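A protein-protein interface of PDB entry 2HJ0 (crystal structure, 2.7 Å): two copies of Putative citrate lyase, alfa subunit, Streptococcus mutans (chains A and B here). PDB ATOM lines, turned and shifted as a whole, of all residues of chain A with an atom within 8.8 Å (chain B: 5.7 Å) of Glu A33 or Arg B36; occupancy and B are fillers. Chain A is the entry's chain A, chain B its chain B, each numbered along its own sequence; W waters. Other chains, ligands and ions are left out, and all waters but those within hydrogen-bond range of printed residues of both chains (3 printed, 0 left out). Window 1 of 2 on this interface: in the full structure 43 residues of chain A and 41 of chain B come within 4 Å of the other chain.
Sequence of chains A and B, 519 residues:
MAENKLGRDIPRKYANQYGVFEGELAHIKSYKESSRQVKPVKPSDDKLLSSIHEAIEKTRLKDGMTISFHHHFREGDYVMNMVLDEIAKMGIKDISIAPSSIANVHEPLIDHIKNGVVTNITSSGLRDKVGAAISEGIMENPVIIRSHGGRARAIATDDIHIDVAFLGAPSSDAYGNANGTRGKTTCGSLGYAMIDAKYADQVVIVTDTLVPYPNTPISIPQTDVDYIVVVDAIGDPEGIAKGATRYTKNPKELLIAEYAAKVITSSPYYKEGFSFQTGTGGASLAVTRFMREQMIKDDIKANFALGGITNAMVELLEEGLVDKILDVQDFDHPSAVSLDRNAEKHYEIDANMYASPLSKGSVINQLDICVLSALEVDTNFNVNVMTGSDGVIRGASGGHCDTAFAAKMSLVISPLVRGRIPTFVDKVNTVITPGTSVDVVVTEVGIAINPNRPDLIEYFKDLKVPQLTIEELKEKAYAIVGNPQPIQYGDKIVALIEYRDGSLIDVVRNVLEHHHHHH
The backbone carbonyl oxygen (O) of Tyr A31 lies within hydrogen-bond range of the backbone NH (N) of Val B38 (2.9 Å). The side-chain amino group of Lys A32 is in hydrogen-bond range of the side-chain hydroxyl of Ser B35. The guanidinium group of Arg B36 lies within salt-bridge range of the side-chain carboxylate of Glu A33. The backbone carbonyl oxygen (O) of Asp B201 sits at hydrogen-bond distance from the side-chain amino group (NZ) of Lys A360 (3.2 Å). The side-chain amino group (NZ) of Lys A360 is in hydrogen-bond range of the backbone carbonyl oxygen (O) of Asp B224, at 3.4 Å. The backbone carbonyl oxygen (O) of Glu A33 lies close to the side-chain hydroxyl (OG) of Ser B35.
The side-chain hydroxyl of Tyr A31 is in hydrogen-bond range of the backbone carbonyl oxygen of Leu A358 (2.8 Å). OH of Tyr A199 lies within hydrogen-bond range of OE2 of Glu A33 (2.5 Å). The backbone carbonyl oxygen (O) of Ser A35 is in hydrogen-bond range of a ring nitrogen (NE2) of His A161, 3.2 Å away. O of Ser B35 sits at hydrogen-bond distance from NE2 of His B161 (3.2 Å). OD1 of Asp B224 is in salt-bridge range of NH2 of Arg B36 (3.4 Å). N of Gln B37 lies within hydrogen-bond range of OD1 of Asp B201 (2.7 Å).
Ser A30 touches Val B38. O of Tyr A31 touches O of Arg B36 (3.8 Å). Tyr A31 touches Gln B37 (O to CA, 3.6 Å). Lys A32 touches Arg B36 (CA to O, 3.7 Å). OE1 of Gln B37 touches CG of Lys A32, at 3.1 Å. Val B38 touches Glu A33 (CG2 to CB, 3.96 Å). Ser A35 touches Ser B35. CG2 of Thr B223 touches ND2 of Asn A352, 3.8 Å away. Lys A360 touches Arg B36. Lys A360 touches Thr B223.
Glu A33 touches just these residues of chain B: Ser B35, Arg B36 and Val B38. Of the printed residues of chain A, Ser B35 touches Lys A32, Glu A33 and Ser A35. Of the printed residues of chain B, Asn A352 touches Thr B223 (3.8 Å). Printed residues of chain B within 4 Å of Lys A32: Ser B35, Arg B36 and Gln B37. Asp A158 touches none of the printed residues of chain B. Asp A159 touches none of the printed residues of chain B.
Hydrophobic or aromatic side chains of chain B within 4 Å of the printed part of chain A: Val B38. Among the printed residues, 16 pairs touch across the chains. Among the printed residues, Asp or Glu carboxylates within 4 Å of a Lys or Arg side-chain nitrogen of the other chain: Glu A33 with Arg B36 (2.7 Å).
Ser A35 touches its own counterpart, Ser B35. Positions printed for both chains: 34, 35, 36, 161, 198 and 199.
Water W3 lies within hydrogen-bond range of the guanidinium group (NH2) of Arg B36, the backbone carbonyl oxygen (O) of Ala B200, the backbone carbonyl oxygen (O) of Ala B197 and the side-chain amino group (NZ) of Lys A360. Water W1 lies within hydrogen-bond range of O of Thr B223 and N of Lys A360. Water W2 bridges O of Asp B201 (3.2 Å) and NZ of Lys A360 (3.4 Å).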
ATOM      1  N   SER A  30      36.609 -20.787 -32.022  1.00  0.00           N
ATOM      2  CA  SER A  30      35.571 -21.028 -31.034  1.00  0.00           C
ATOM      3  C   SER A  30      34.866 -19.755 -30.569  1.00  0.00           C
ATOM      4  O   SER A  30      35.479 -18.687 -30.473  1.00  0.00           O
ATOM      5  CB  SER A  30      36.159 -21.769 -29.828  1.00  0.00           C
ATOM      6  OG  SER A  30      37.053 -20.939 -29.103  1.00  0.00           O
ATOM      7  N   TYR A  31      33.571 -19.878 -30.280  1.00  0.00           N
ATOM      8  CA  TYR A  31      32.765 -18.747 -29.817  1.00  0.00           C
ATOM      9  C   TYR A  31      31.713 -19.187 -28.803  1.00  0.00           C
ATOM     10  O   TYR A  31      31.388 -20.366 -28.708  1.00  0.00           O
ATOM     11  CB  TYR A  31      32.075 -18.080 -31.005  1.00  0.00           C
ATOM     12  CG  TYR A  31      31.000 -18.924 -31.647  1.00  0.00           C
ATOM     13  CD1 TYR A  31      29.713 -18.964 -31.125  1.00  0.00           C
ATOM     14  CD2 TYR A  31      31.279 -19.698 -32.765  1.00  0.00           C
ATOM     15  CE1 TYR A  31      28.729 -19.756 -31.704  1.00  0.00           C
ATOM     16  CE2 TYR A  31      30.308 -20.492 -33.352  1.00  0.00           C
ATOM     17  CZ  TYR A  31      29.032 -20.521 -32.821  1.00  0.00           C
ATOM     18  OH  TYR A  31      28.070 -21.310 -33.410  1.00  0.00           O
ATOM     19  N   LYS A  32      31.189 -18.227 -28.051  1.00  0.00           N
ATOM     20  CA  LYS A  32      30.159 -18.499 -27.062  1.00  0.00           C
ATOM     21  C   LYS A  32      28.808 -18.312 -27.731  1.00  0.00           C
ATOM     22  O   LYS A  32      28.431 -17.194 -28.098  1.00  0.00           O
ATOM     23  CB  LYS A  32      30.277 -17.534 -25.888  1.00  0.00           C
ATOM     24  CG  LYS A  32      30.875 -18.138 -24.642  1.00  0.00           C
ATOM     25  CD  LYS A  32      29.809 -18.749 -23.740  1.00  0.00           C
ATOM     26  CE  LYS A  32      28.909 -17.681 -23.123  1.00  0.00           C
ATOM     27  NZ  LYS A  32      28.056 -16.964 -24.124  1.00  0.00           N
ATOM     28  N   GLU A  33      28.089 -19.412 -27.910  1.00  0.00           N
ATOM     29  CA  GLU A  33      26.780 -19.369 -28.533  1.00  0.00           C
ATOM     30  C   GLU A  33      25.880 -18.410 -27.774  1.00  0.00           C
ATOM     31  O   GLU A  33      26.043 -18.185 -26.571  1.00  0.00           O
ATOM     32  CB  GLU A  33      26.160 -20.765 -28.548  1.00  0.00           C
ATOM     33  CG  GLU A  33      24.756 -20.825 -29.134  1.00  0.00           C
ATOM     34  CD  GLU A  33      24.161 -22.220 -29.074  1.00  0.00           C
ATOM     35  OE1 GLU A  33      24.151 -22.825 -27.978  1.00  0.00           O
ATOM     36  OE2 GLU A  33      23.700 -22.711 -30.122  1.00  0.00           O
ATOM     37  N   SER A  34      24.929 -17.833 -28.490  1.00  0.00           N
ATOM     38  CA  SER A  34      23.981 -16.902 -27.900  1.00  0.00           C
ATOM     39  C   SER A  34      23.060 -17.623 -26.907  1.00  0.00           C
ATOM     40  O   SER A  34      22.703 -18.776 -27.116  1.00  0.00           O
ATOM     41  CB  SER A  34      23.164 -16.271 -29.033  1.00  0.00           C
ATOM     42  OG  SER A  34      22.042 -15.550 -28.555  1.00  0.00           O
ATOM     43  N   SER A  35      22.703 -16.960 -25.815  1.00  0.00           N
ATOM     44  CA  SER A  35      21.776 -17.547 -24.841  1.00  0.00           C
ATOM     45  C   SER A  35      20.602 -16.562 -24.737  1.00  0.00           C
ATOM     46  O   SER A  35      20.781 -15.350 -24.884  1.00  0.00           O
ATOM     47  CB  SER A  35      22.436 -17.735 -23.467  1.00  0.00           C
ATOM     48  OG  SER A  35      22.762 -16.487 -22.872  1.00  0.00           O
ATOM     49  N   ARG A  36      19.411 -17.083 -24.469  1.00  0.00           N
ATOM     50  CA  ARG A  36      18.217 -16.260 -24.387  1.00  0.00           C
ATOM     51  C   ARG A  36      17.738 -16.031 -22.961  1.00  0.00           C
ATOM     52  O   ARG A  36      18.138 -16.744 -22.047  1.00  0.00           O
ATOM     53  CB  ARG A  36      17.103 -16.916 -25.215  1.00  0.00           C
ATOM     54  CG  ARG A  36      16.913 -18.368 -24.867  1.00  0.00           C
ATOM     55  CD  ARG A  36      16.121 -19.163 -25.894  1.00  0.00           C
ATOM     56  NE  ARG A  36      16.070 -20.562 -25.452  1.00  0.00           N
ATOM     57  CZ  ARG A  36      14.971 -21.309 -25.398  1.00  0.00           C
ATOM     58  NH1 ARG A  36      15.051 -22.563 -24.966  1.00  0.00           N
ATOM     59  NH2 ARG A  36      13.802 -20.807 -25.778  1.00  0.00           N
ATOM     60  N   ALA A 152      21.812 -17.013 -39.800  1.00  0.00           N
ATOM     61  CA  ALA A 152      21.903 -18.040 -38.786  1.00  0.00           C
ATOM     62  C   ALA A 152      23.197 -17.817 -37.996  1.00  0.00           C
ATOM     63  O   ALA A 152      23.191 -17.918 -36.777  1.00  0.00           O
ATOM     64  CB  ALA A 152      21.883 -19.425 -39.437  1.00  0.00           C
ATOM     65  N   ARG A 153      24.295 -17.502 -38.681  1.00  0.00           N
ATOM     66  CA  ARG A 153      25.559 -17.264 -37.993  1.00  0.00           C
ATOM     67  C   ARG A 153      25.425 -16.092 -37.023  1.00  0.00           C
ATOM     68  O   ARG A 153      25.774 -16.212 -35.850  1.00  0.00           O
ATOM     69  CB  ARG A 153      26.683 -16.956 -38.977  1.00  0.00           C
ATOM     70  CG  ARG A 153      28.039 -16.742 -38.295  1.00  0.00           C
ATOM     71  CD  ARG A 153      28.782 -15.534 -38.870  1.00  0.00           C
ATOM     72  NE  ARG A 153      28.141 -14.268 -38.518  1.00  0.00           N
ATOM     73  CZ  ARG A 153      27.747 -13.356 -39.402  1.00  0.00           C
ATOM     74  NH1 ARG A 153      27.926 -13.571 -40.695  1.00  0.00           N
ATOM     75  NH2 ARG A 153      27.180 -12.227 -39.000  1.00  0.00           N
ATOM     76  N   ALA A 154      24.915 -14.961 -37.511  1.00  0.00           N
ATOM     77  CA  ALA A 154      24.747 -13.777 -36.661  1.00  0.00           C
ATOM     78  C   ALA A 154      23.922 -14.051 -35.411  1.00  0.00           C
ATOM     79  O   ALA A 154      24.336 -13.698 -34.306  1.00  0.00           O
ATOM     80  CB  ALA A 154      24.121 -12.641 -37.437  1.00  0.00           C
ATOM     81  N   ILE A 155      22.762 -14.676 -35.577  1.00  0.00           N
ATOM     82  CA  ILE A 155      21.912 -14.958 -34.441  1.00  0.00           C
ATOM     83  C   ILE A 155      22.611 -15.864 -33.436  1.00  0.00           C
ATOM     84  O   ILE A 155      22.523 -15.642 -32.236  1.00  0.00           O
ATOM     85  CB  ILE A 155      20.579 -15.575 -34.900  1.00  0.00           C
ATOM     86  CG1 ILE A 155      19.862 -14.574 -35.808  1.00  0.00           C
ATOM     87  CG2 ILE A 155      19.712 -15.942 -33.694  1.00  0.00           C
ATOM     88  CD1 ILE A 155      18.527 -15.027 -36.335  1.00  0.00           C
ATOM     89  N   ALA A 156      23.342 -16.855 -33.913  1.00  0.00           N
ATOM     90  CA  ALA A 156      24.022 -17.763 -33.005  1.00  0.00           C
ATOM     91  C   ALA A 156      25.245 -17.149 -32.332  1.00  0.00           C
ATOM     92  O   ALA A 156      25.563 -17.486 -31.197  1.00  0.00           O
ATOM     93  CB  ALA A 156      24.415 -19.025 -33.751  1.00  0.00           C
ATOM     94  N   THR A 157      25.929 -16.260 -33.041  1.00  0.00           N
ATOM     95  CA  THR A 157      27.115 -15.585 -32.528  1.00  0.00           C
ATOM     96  C   THR A 157      26.719 -14.483 -31.559  1.00  0.00           C
ATOM     97  O   THR A 157      27.550 -13.940 -30.835  1.00  0.00           O
ATOM     98  CB  THR A 157      27.897 -14.950 -33.663  1.00  0.00           C
ATOM     99  OG1 THR A 157      28.238 -15.965 -34.606  1.00  0.00           O
ATOM    100  CG2 THR A 157      29.176 -14.308 -33.143  1.00  0.00           C
ATOM    101  N   ASP A 158      25.433 -14.166 -31.562  1.00  0.00           N
ATOM    102  CA  ASP A 158      24.862 -13.126 -30.719  1.00  0.00           C
ATOM    103  C   ASP A 158      25.272 -11.726 -31.157  1.00  0.00           C
ATOM    104  O   ASP A 158      25.071 -10.764 -30.418  1.00  0.00           O
ATOM    105  CB  ASP A 158      25.237 -13.318 -29.241  1.00  0.00           C
ATOM    106  CG  ASP A 158      24.208 -12.697 -28.285  1.00  0.00           C
ATOM    107  OD1 ASP A 158      24.425 -12.739 -27.053  1.00  0.00           O
ATOM    108  OD2 ASP A 158      23.176 -12.179 -28.764  1.00  0.00           O
ATOM    109  N   ASP A 159      25.840 -11.575 -32.343  1.00  0.00           N
ATOM    110  CA  ASP A 159      26.186 -10.228 -32.727  1.00  0.00           C
ATOM    111  C   ASP A 159      24.909  -9.568 -33.211  1.00  0.00           C
ATOM    112  O   ASP A 159      24.930  -8.515 -33.834  1.00  0.00           O
ATOM    113  CB  ASP A 159      27.303 -10.207 -33.775  1.00  0.00           C
ATOM    114  CG  ASP A 159      26.995 -11.052 -34.953  1.00  0.00           C
ATOM    115  OD1 ASP A 159      27.940 -11.405 -35.701  1.00  0.00           O
ATOM    116  OD2 ASP A 159      25.795 -11.358 -35.128  1.00  0.00           O
ATOM    117  N   HIS A 161      20.525  -9.915 -31.649  1.00  0.00           N
ATOM    118  CA  HIS A 161      19.686 -10.614 -30.674  1.00  0.00           C
ATOM    119  C   HIS A 161      18.207 -10.265 -30.808  1.00  0.00           C
ATOM    120  O   HIS A 161      17.815  -9.099 -30.702  1.00  0.00           O
ATOM    121  CB  HIS A 161      20.188 -10.284 -29.270  1.00  0.00           C
ATOM    122  CG  HIS A 161      19.871 -11.325 -28.248  1.00  0.00           C
ATOM    123  ND1 HIS A 161      18.683 -11.351 -27.553  1.00  0.00           N
ATOM    124  CD2 HIS A 161      20.590 -12.387 -27.806  1.00  0.00           C
ATOM    125  CE1 HIS A 161      18.681 -12.384 -26.727  1.00  0.00           C
ATOM    126  NE2 HIS A 161      19.827 -13.027 -26.861  1.00  0.00           N
ATOM    127  N   ILE A 195      15.040 -21.430 -36.278  1.00  0.00           N
ATOM    128  CA  ILE A 195      16.196 -20.854 -35.626  1.00  0.00           C
ATOM    129  C   ILE A 195      15.760 -19.672 -34.770  1.00  0.00           C
ATOM    130  O   ILE A 195      16.290 -19.461 -33.695  1.00  0.00           O
ATOM    131  CB  ILE A 195      17.235 -20.425 -36.648  1.00  0.00           C
ATOM    132  CG1 ILE A 195      18.391 -19.734 -35.946  1.00  0.00           C
ATOM    133  CG2 ILE A 195      16.612 -19.514 -37.673  1.00  0.00           C
ATOM    134  CD1 ILE A 195      19.501 -19.384 -36.887  1.00  0.00           C
ATOM    135  N   LYS A 198      14.478 -20.627 -31.492  1.00  0.00           N
ATOM    136  CA  LYS A 198      15.520 -21.245 -30.692  1.00  0.00           C
ATOM    137  C   LYS A 198      16.427 -20.224 -29.997  1.00  0.00           C
ATOM    138  O   LYS A 198      16.910 -20.467 -28.898  1.00  0.00           O
ATOM    139  CB  LYS A 198      16.323 -22.168 -31.601  1.00  0.00           C
ATOM    140  CG  LYS A 198      17.460 -22.916 -30.960  1.00  0.00           C
ATOM    141  CD  LYS A 198      18.019 -23.951 -31.952  1.00  0.00           C
ATOM    142  CE  LYS A 198      16.907 -24.922 -32.436  1.00  0.00           C
ATOM    143  NZ  LYS A 198      17.339 -25.949 -33.444  1.00  0.00           N
ATOM    144  N   TYR A 199      16.634 -19.072 -30.622  1.00  0.00           N
ATOM    145  CA  TYR A 199      17.498 -18.065 -30.034  1.00  0.00           C
ATOM    146  C   TYR A 199      16.825 -16.788 -29.537  1.00  0.00           C
ATOM    147  O   TYR A 199      17.427 -16.020 -28.796  1.00  0.00           O
ATOM    148  CB  TYR A 199      18.581 -17.703 -31.036  1.00  0.00           C
ATOM    149  CG  TYR A 199      19.535 -18.825 -31.278  1.00  0.00           C
ATOM    150  CD1 TYR A 199      20.537 -19.130 -30.349  1.00  0.00           C
ATOM    151  CD2 TYR A 199      19.435 -19.601 -32.427  1.00  0.00           C
ATOM    152  CE1 TYR A 199      21.423 -20.196 -30.570  1.00  0.00           C
ATOM    153  CE2 TYR A 199      20.301 -20.662 -32.662  1.00  0.00           C
ATOM    154  CZ  TYR A 199      21.294 -20.958 -31.734  1.00  0.00           C
ATOM    155  OH  TYR A 199      22.151 -22.009 -31.967  1.00  0.00           O
ATOM    156  N   ASN A 352      20.183 -23.120 -39.693  1.00  0.00           N
ATOM    157  CA  ASN A 352      21.527 -23.223 -39.156  1.00  0.00           C
ATOM    158  C   ASN A 352      22.170 -24.518 -39.606  1.00  0.00           C
ATOM    159  O   ASN A 352      23.288 -24.522 -40.123  1.00  0.00           O
ATOM    160  CB  ASN A 352      21.537 -23.159 -37.632  1.00  0.00           C
ATOM    161  CG  ASN A 352      22.955 -23.044 -37.068  1.00  0.00           C
ATOM    162  OD1 ASN A 352      23.650 -22.038 -37.279  1.00  0.00           O
ATOM    163  ND2 ASN A 352      23.395 -24.082 -36.361  1.00  0.00           N
ATOM    164  N   LEU A 358      29.529 -21.062 -39.254  1.00  0.00           N
ATOM    165  CA  LEU A 358      30.049 -21.235 -37.906  1.00  0.00           C
ATOM    166  C   LEU A 358      29.231 -22.197 -37.085  1.00  0.00           C
ATOM    167  O   LEU A 358      28.584 -21.804 -36.118  1.00  0.00           O
ATOM    168  CB  LEU A 358      30.093 -19.907 -37.168  1.00  0.00           C
ATOM    169  CG  LEU A 358      31.276 -19.013 -37.490  1.00  0.00           C
ATOM    170  CD1 LEU A 358      31.256 -17.812 -36.563  1.00  0.00           C
ATOM    171  CD2 LEU A 358      32.560 -19.804 -37.320  1.00  0.00           C
ATOM    172  N   SER A 359      29.271 -23.465 -37.452  1.00  0.00           N
ATOM    173  CA  SER A 359      28.503 -24.471 -36.735  1.00  0.00           C
ATOM    174  C   SER A 359      29.377 -25.690 -36.557  1.00  0.00           C
ATOM    175  O   SER A 359      30.553 -25.683 -36.900  1.00  0.00           O
ATOM    176  CB  SER A 359      27.298 -24.878 -37.565  1.00  0.00           C
ATOM    177  OG  SER A 359      27.740 -25.627 -38.687  1.00  0.00           O
ATOM    178  N   LYS A 360      28.787 -26.749 -36.033  1.00  0.00           N
ATOM    179  CA  LYS A 360      29.528 -27.966 -35.863  1.00  0.00           C
ATOM    180  C   LYS A 360      29.405 -28.742 -37.146  1.00  0.00           C
ATOM    181  O   LYS A 360      29.926 -29.850 -37.260  1.00  0.00           O
ATOM    182  CB  LYS A 360      28.987 -28.775 -34.696  1.00  0.00           C
ATOM    183  CG  LYS A 360      29.193 -28.054 -33.390  1.00  0.00           C
ATOM    184  CD  LYS A 360      28.973 -28.969 -32.225  1.00  0.00           C
ATOM    185  CE  LYS A 360      29.223 -28.237 -30.940  1.00  0.00           C
ATOM    186  NZ  LYS A 360      29.084 -29.158 -29.801  1.00  0.00           N
ATOM    187  N   SER B  34      21.520 -21.362 -20.230  1.00  0.00           N
ATOM    188  CA  SER B  34      22.926 -21.696 -20.398  1.00  0.00           C
ATOM    189  C   SER B  34      23.322 -21.618 -21.877  1.00  0.00           C
ATOM    190  O   SER B  34      22.525 -21.934 -22.750  1.00  0.00           O
ATOM    191  CB  SER B  34      23.163 -23.112 -19.862  1.00  0.00           C
ATOM    192  OG  SER B  34      24.433 -23.615 -20.238  1.00  0.00           O
ATOM    193  N   SER B  35      24.540 -21.176 -22.160  1.00  0.00           N
ATOM    194  CA  SER B  35      25.021 -21.109 -23.539  1.00  0.00           C
ATOM    195  C   SER B  35      26.305 -21.943 -23.563  1.00  0.00           C
ATOM    196  O   SER B  35      27.026 -22.011 -22.562  1.00  0.00           O
ATOM    197  CB  SER B  35      25.315 -19.664 -23.962  1.00  0.00           C
ATOM    198  OG  SER B  35      26.379 -19.108 -23.212  1.00  0.00           O
ATOM    199  N   ARG B  36      26.585 -22.568 -24.700  1.00  0.00           N
ATOM    200  CA  ARG B  36      27.760 -23.417 -24.842  1.00  0.00           C
ATOM    201  C   ARG B  36      28.888 -22.792 -25.663  1.00  0.00           C
ATOM    202  O   ARG B  36      28.681 -21.845 -26.416  1.00  0.00           O
ATOM    203  CB  ARG B  36      27.343 -24.741 -25.479  1.00  0.00           C
ATOM    204  CG  ARG B  36      26.592 -24.545 -26.776  1.00  0.00           C
ATOM    205  CD  ARG B  36      25.788 -25.752 -27.231  1.00  0.00           C
ATOM    206  NE  ARG B  36      25.021 -25.378 -28.418  1.00  0.00           N
ATOM    207  CZ  ARG B  36      24.990 -26.069 -29.551  1.00  0.00           C
ATOM    208  NH1 ARG B  36      24.268 -25.624 -30.571  1.00  0.00           N
ATOM    209  NH2 ARG B  36      25.672 -27.203 -29.660  1.00  0.00           N
ATOM    210  N   GLN B  37      30.089 -23.336 -25.489  1.00  0.00           N
ATOM    211  CA  GLN B  37      31.277 -22.884 -26.198  1.00  0.00           C
ATOM    212  C   GLN B  37      31.432 -23.751 -27.426  1.00  0.00           C
ATOM    213  O   GLN B  37      31.982 -24.852 -27.353  1.00  0.00           O
ATOM    214  CB  GLN B  37      32.514 -23.031 -25.318  1.00  0.00           C
ATOM    215  CG  GLN B  37      32.788 -21.831 -24.434  1.00  0.00           C
ATOM    216  CD  GLN B  37      33.521 -20.729 -25.174  1.00  0.00           C
ATOM    217  OE1 GLN B  37      33.651 -19.605 -24.674  1.00  0.00           O
ATOM    218  NE2 GLN B  37      34.019 -21.048 -26.371  1.00  0.00           N
ATOM    219  N   VAL B  38      30.947 -23.241 -28.554  1.00  0.00           N
ATOM    220  CA  VAL B  38      30.974 -23.946 -29.832  1.00  0.00           C
ATOM    221  C   VAL B  38      32.301 -23.853 -30.575  1.00  0.00           C
ATOM    222  O   VAL B  38      32.908 -22.792 -30.634  1.00  0.00           O
ATOM    223  CB  VAL B  38      29.886 -23.382 -30.760  1.00  0.00           C
ATOM    224  CG1 VAL B  38      29.919 -24.085 -32.091  1.00  0.00           C
ATOM    225  CG2 VAL B  38      28.532 -23.522 -30.111  1.00  0.00           C
ATOM    226  N   HIS B 161      27.559 -27.263 -15.689  1.00  0.00           N
ATOM    227  CA  HIS B 161      27.935 -27.132 -17.095  1.00  0.00           C
ATOM    228  C   HIS B 161      28.765 -28.321 -17.597  1.00  0.00           C
ATOM    229  O   HIS B 161      29.827 -28.640 -17.057  1.00  0.00           O
ATOM    230  CB  HIS B 161      28.693 -25.811 -17.283  1.00  0.00           C
ATOM    231  CG  HIS B 161      28.609 -25.245 -18.670  1.00  0.00           C
ATOM    232  ND1 HIS B 161      29.471 -25.614 -19.683  1.00  0.00           N
ATOM    233  CD2 HIS B 161      27.752 -24.351 -19.217  1.00  0.00           C
ATOM    234  CE1 HIS B 161      29.149 -24.971 -20.792  1.00  0.00           C
ATOM    235  NE2 HIS B 161      28.109 -24.199 -20.538  1.00  0.00           N
ATOM    236  N   ALA B 197      23.358 -33.091 -25.472  1.00  0.00           N
ATOM    237  CA  ALA B 197      23.917 -32.617 -26.729  1.00  0.00           C
ATOM    238  C   ALA B 197      23.514 -31.194 -27.062  1.00  0.00           C
ATOM    239  O   ALA B 197      24.105 -30.563 -27.931  1.00  0.00           O
ATOM    240  CB  ALA B 197      23.507 -33.537 -27.853  1.00  0.00           C
ATOM    241  N   LYS B 198      22.514 -30.691 -26.364  1.00  0.00           N
ATOM    242  CA  LYS B 198      22.019 -29.363 -26.618  1.00  0.00           C
ATOM    243  C   LYS B 198      22.727 -28.308 -25.769  1.00  0.00           C
ATOM    244  O   LYS B 198      22.903 -27.166 -26.198  1.00  0.00           O
ATOM    245  CB  LYS B 198      20.513 -29.371 -26.357  1.00  0.00           C
ATOM    246  CG  LYS B 198      19.785 -28.063 -26.534  1.00  0.00           C
ATOM    247  CD  LYS B 198      18.270 -28.291 -26.456  1.00  0.00           C
ATOM    248  CE  LYS B 198      17.794 -29.316 -27.524  1.00  0.00           C
ATOM    249  NZ  LYS B 198      16.325 -29.655 -27.477  1.00  0.00           N
ATOM    250  N   TYR B 199      23.159 -28.684 -24.572  1.00  0.00           N
ATOM    251  CA  TYR B 199      23.810 -27.722 -23.696  1.00  0.00           C
ATOM    252  C   TYR B 199      25.285 -27.956 -23.434  1.00  0.00           C
ATOM    253  O   TYR B 199      25.965 -27.062 -22.945  1.00  0.00           O
ATOM    254  CB  TYR B 199      23.067 -27.667 -22.370  1.00  0.00           C
ATOM    255  CG  TYR B 199      21.693 -27.079 -22.499  1.00  0.00           C
ATOM    256  CD1 TYR B 199      21.510 -25.695 -22.614  1.00  0.00           C
ATOM    257  CD2 TYR B 199      20.566 -27.901 -22.511  1.00  0.00           C
ATOM    258  CE1 TYR B 199      20.236 -25.151 -22.733  1.00  0.00           C
ATOM    259  CE2 TYR B 199      19.294 -27.366 -22.629  1.00  0.00           C
ATOM    260  CZ  TYR B 199      19.138 -25.993 -22.739  1.00  0.00           C
ATOM    261  OH  TYR B 199      17.880 -25.468 -22.841  1.00  0.00           O
ATOM    262  N   ALA B 200      25.780 -29.143 -23.760  1.00  0.00           N
ATOM    263  CA  ALA B 200      27.177 -29.465 -23.527  1.00  0.00           C
ATOM    264  C   ALA B 200      28.078 -28.688 -24.471  1.00  0.00           C
ATOM    265  O   ALA B 200      27.667 -28.330 -25.579  1.00  0.00           O
ATOM    266  CB  ALA B 200      27.396 -30.949 -23.699  1.00  0.00           C
ATOM    267  N   ASP B 201      29.307 -28.417 -24.031  1.00  0.00           N
ATOM    268  CA  ASP B 201      30.238 -27.682 -24.877  1.00  0.00           C
ATOM    269  C   ASP B 201      30.681 -28.562 -26.023  1.00  0.00           C
ATOM    270  O   ASP B 201      30.572 -28.184 -27.187  1.00  0.00           O
ATOM    271  CB  ASP B 201      31.452 -27.198 -24.083  1.00  0.00           C
ATOM    272  CG  ASP B 201      31.173 -25.912 -23.313  1.00  0.00           C
ATOM    273  OD1 ASP B 201      30.169 -25.234 -23.629  1.00  0.00           O
ATOM    274  OD2 ASP B 201      31.966 -25.577 -22.401  1.00  0.00           O
ATOM    275  N   THR B 223      24.573 -30.559 -35.871  1.00  0.00           N
ATOM    276  CA  THR B 223      24.934 -29.270 -35.305  1.00  0.00           C
ATOM    277  C   THR B 223      25.194 -29.299 -33.813  1.00  0.00           C
ATOM    278  O   THR B 223      25.622 -28.300 -33.243  1.00  0.00           O
ATOM    279  CB  THR B 223      23.861 -28.205 -35.572  1.00  0.00           C
ATOM    280  OG1 THR B 223      22.571 -28.731 -35.242  1.00  0.00           O
ATOM    281  CG2 THR B 223      23.892 -27.772 -37.022  1.00  0.00           C
ATOM    282  N   ASP B 224      24.930 -30.428 -33.173  1.00  0.00           N
ATOM    283  CA  ASP B 224      25.180 -30.536 -31.740  1.00  0.00           C
ATOM    284  C   ASP B 224      26.327 -31.493 -31.465  1.00  0.00           C
ATOM    285  O   ASP B 224      26.759 -31.636 -30.328  1.00  0.00           O
ATOM    286  CB  ASP B 224      23.947 -31.057 -30.999  1.00  0.00           C
ATOM    287  CG  ASP B 224      22.841 -30.019 -30.886  1.00  0.00           C
ATOM    288  OD1 ASP B 224      23.095 -28.819 -31.157  1.00  0.00           O
ATOM    289  OD2 ASP B 224      21.714 -30.403 -30.508  1.00  0.00           O
HETATM  290  O   HOH W   1      26.201 -25.575 -34.411  1.00  0.00           O
HETATM  291  O   HOH W   2      31.943 -27.382 -29.917  1.00  0.00           O
HETATM  292  O   HOH W   3      26.627 -29.023 -27.992  1.00  0.00           O
